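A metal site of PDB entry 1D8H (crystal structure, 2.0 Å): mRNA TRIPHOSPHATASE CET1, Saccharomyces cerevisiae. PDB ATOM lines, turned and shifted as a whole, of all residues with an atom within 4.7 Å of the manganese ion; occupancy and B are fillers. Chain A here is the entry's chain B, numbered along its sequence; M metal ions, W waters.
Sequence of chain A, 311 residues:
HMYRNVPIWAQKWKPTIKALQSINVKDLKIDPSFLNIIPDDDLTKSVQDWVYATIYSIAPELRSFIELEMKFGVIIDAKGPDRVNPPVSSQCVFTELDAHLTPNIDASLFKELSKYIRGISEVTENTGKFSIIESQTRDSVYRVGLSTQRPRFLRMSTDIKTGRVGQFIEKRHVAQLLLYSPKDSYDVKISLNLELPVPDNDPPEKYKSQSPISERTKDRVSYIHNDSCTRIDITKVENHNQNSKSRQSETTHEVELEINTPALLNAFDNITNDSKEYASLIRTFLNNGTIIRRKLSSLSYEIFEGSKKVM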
ATOM      1  N   GLU A  67     -25.620  24.625   7.343  1.00  0.00           N
ATOM      2  CA  GLU A  67     -24.586  25.562   6.630  1.00  0.00           C
ATOM      3  C   GLU A  67     -23.681  24.587   5.847  1.00  0.00           C
ATOM      4  O   GLU A  67     -23.213  23.669   6.462  1.00  0.00           O
ATOM      5  CB  GLU A  67     -23.735  26.324   7.632  1.00  0.00           C
ATOM      6  CG  GLU A  67     -22.415  26.861   6.932  1.00  0.00           C
ATOM      7  CD  GLU A  67     -21.517  27.303   8.134  1.00  0.00           C
ATOM      8  OE1 GLU A  67     -20.819  26.449   8.732  1.00  0.00           O
ATOM      9  OE2 GLU A  67     -21.633  28.515   8.433  1.00  0.00           O
ATOM     10  N   GLU A  69     -20.373  24.230   3.578  1.00  0.00           N
ATOM     11  CA  GLU A  69     -19.323  25.070   3.026  1.00  0.00           C
ATOM     12  C   GLU A  69     -18.007  24.375   2.828  1.00  0.00           C
ATOM     13  O   GLU A  69     -17.836  23.356   3.470  1.00  0.00           O
ATOM     14  CB  GLU A  69     -19.000  26.197   4.073  1.00  0.00           C
ATOM     15  CG  GLU A  69     -18.740  25.741   5.481  1.00  0.00           C
ATOM     16  CD  GLU A  69     -18.449  26.888   6.476  1.00  0.00           C
ATOM     17  OE1 GLU A  69     -17.465  26.741   7.313  1.00  0.00           O
ATOM     18  OE2 GLU A  69     -19.007  27.982   6.443  1.00  0.00           O
ATOM     19  N   LYS A 171     -23.375  26.181  17.291  1.00  0.00           N
ATOM     20  CA  LYS A 171     -22.934  25.636  16.053  1.00  0.00           C
ATOM     21  C   LYS A 171     -22.591  24.165  16.149  1.00  0.00           C
ATOM     22  O   LYS A 171     -21.682  23.819  16.932  1.00  0.00           O
ATOM     23  CB  LYS A 171     -21.732  26.390  15.449  1.00  0.00           C
ATOM     24  CG  LYS A 171     -21.979  26.453  13.916  1.00  0.00           C
ATOM     25  CD  LYS A 171     -20.795  27.090  13.245  1.00  0.00           C
ATOM     26  CE  LYS A 171     -21.298  27.809  12.001  1.00  0.00           C
ATOM     27  NZ  LYS A 171     -20.120  28.002  11.117  1.00  0.00           N
ATOM     28  N   ASP A 233     -16.255  33.673   1.547  1.00  0.00           N
ATOM     29  CA  ASP A 233     -16.009  34.506   2.723  1.00  0.00           C
ATOM     30  C   ASP A 233     -14.504  34.620   2.827  1.00  0.00           C
ATOM     31  O   ASP A 233     -13.964  33.530   3.033  1.00  0.00           O
ATOM     32  CB  ASP A 233     -16.624  33.957   4.060  1.00  0.00           C
ATOM     33  CG  ASP A 233     -18.105  34.180   4.157  1.00  0.00           C
ATOM     34  OD1 ASP A 233     -18.851  33.426   4.937  1.00  0.00           O
ATOM     35  OD2 ASP A 233     -18.647  35.132   3.545  1.00  0.00           O
ATOM     36  N   GLU A 258     -19.421  28.919   0.607  1.00  0.00           N
ATOM     37  CA  GLU A 258     -20.733  28.435   1.083  1.00  0.00           C
ATOM     38  C   GLU A 258     -21.779  28.430   0.023  1.00  0.00           C
ATOM     39  O   GLU A 258     -21.978  29.363  -0.703  1.00  0.00           O
ATOM     40  CB  GLU A 258     -21.449  29.318   2.074  1.00  0.00           C
ATOM     41  CG  GLU A 258     -21.047  29.441   3.488  1.00  0.00           C
ATOM     42  CD  GLU A 258     -21.894  30.456   4.276  1.00  0.00           C
ATOM     43  OE1 GLU A 258     -22.894  31.078   4.000  1.00  0.00           O
ATOM     44  OE2 GLU A 258     -21.514  30.913   5.368  1.00  0.00           O
HETATM   45 MN    MN M   1     -20.039  29.939   6.862  1.00  0.00          MN
HETATM   46  O   HOH W   1     -18.741  29.418   8.325  1.00  0.00           O
HETATM   47  O   HOH W   2     -17.381  31.070   6.428  1.00  0.00           O
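OE1 of Glu 67 lies within salt-bridge range of NZ of Lys 171 (2.9 Å).
The nearest printed residue that does not touch the manganese ion is Asp 233 (4.2 Å).
The manganese ion is bound by water W1 (2.0 Å), the side-chain carboxylate of Glu 69 (2.3 Å), the side-chain carboxylate of Glu 258 (2.3 Å) and the side-chain carboxylate of Glu 67 (2.7 Å). Slightly farther from the manganese ion lies water W2 (2.9 Å).
Water W1 bridges OE1 of Glu 69 (3.1 Å) and NZ of Lys 171 (3.4 Å).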
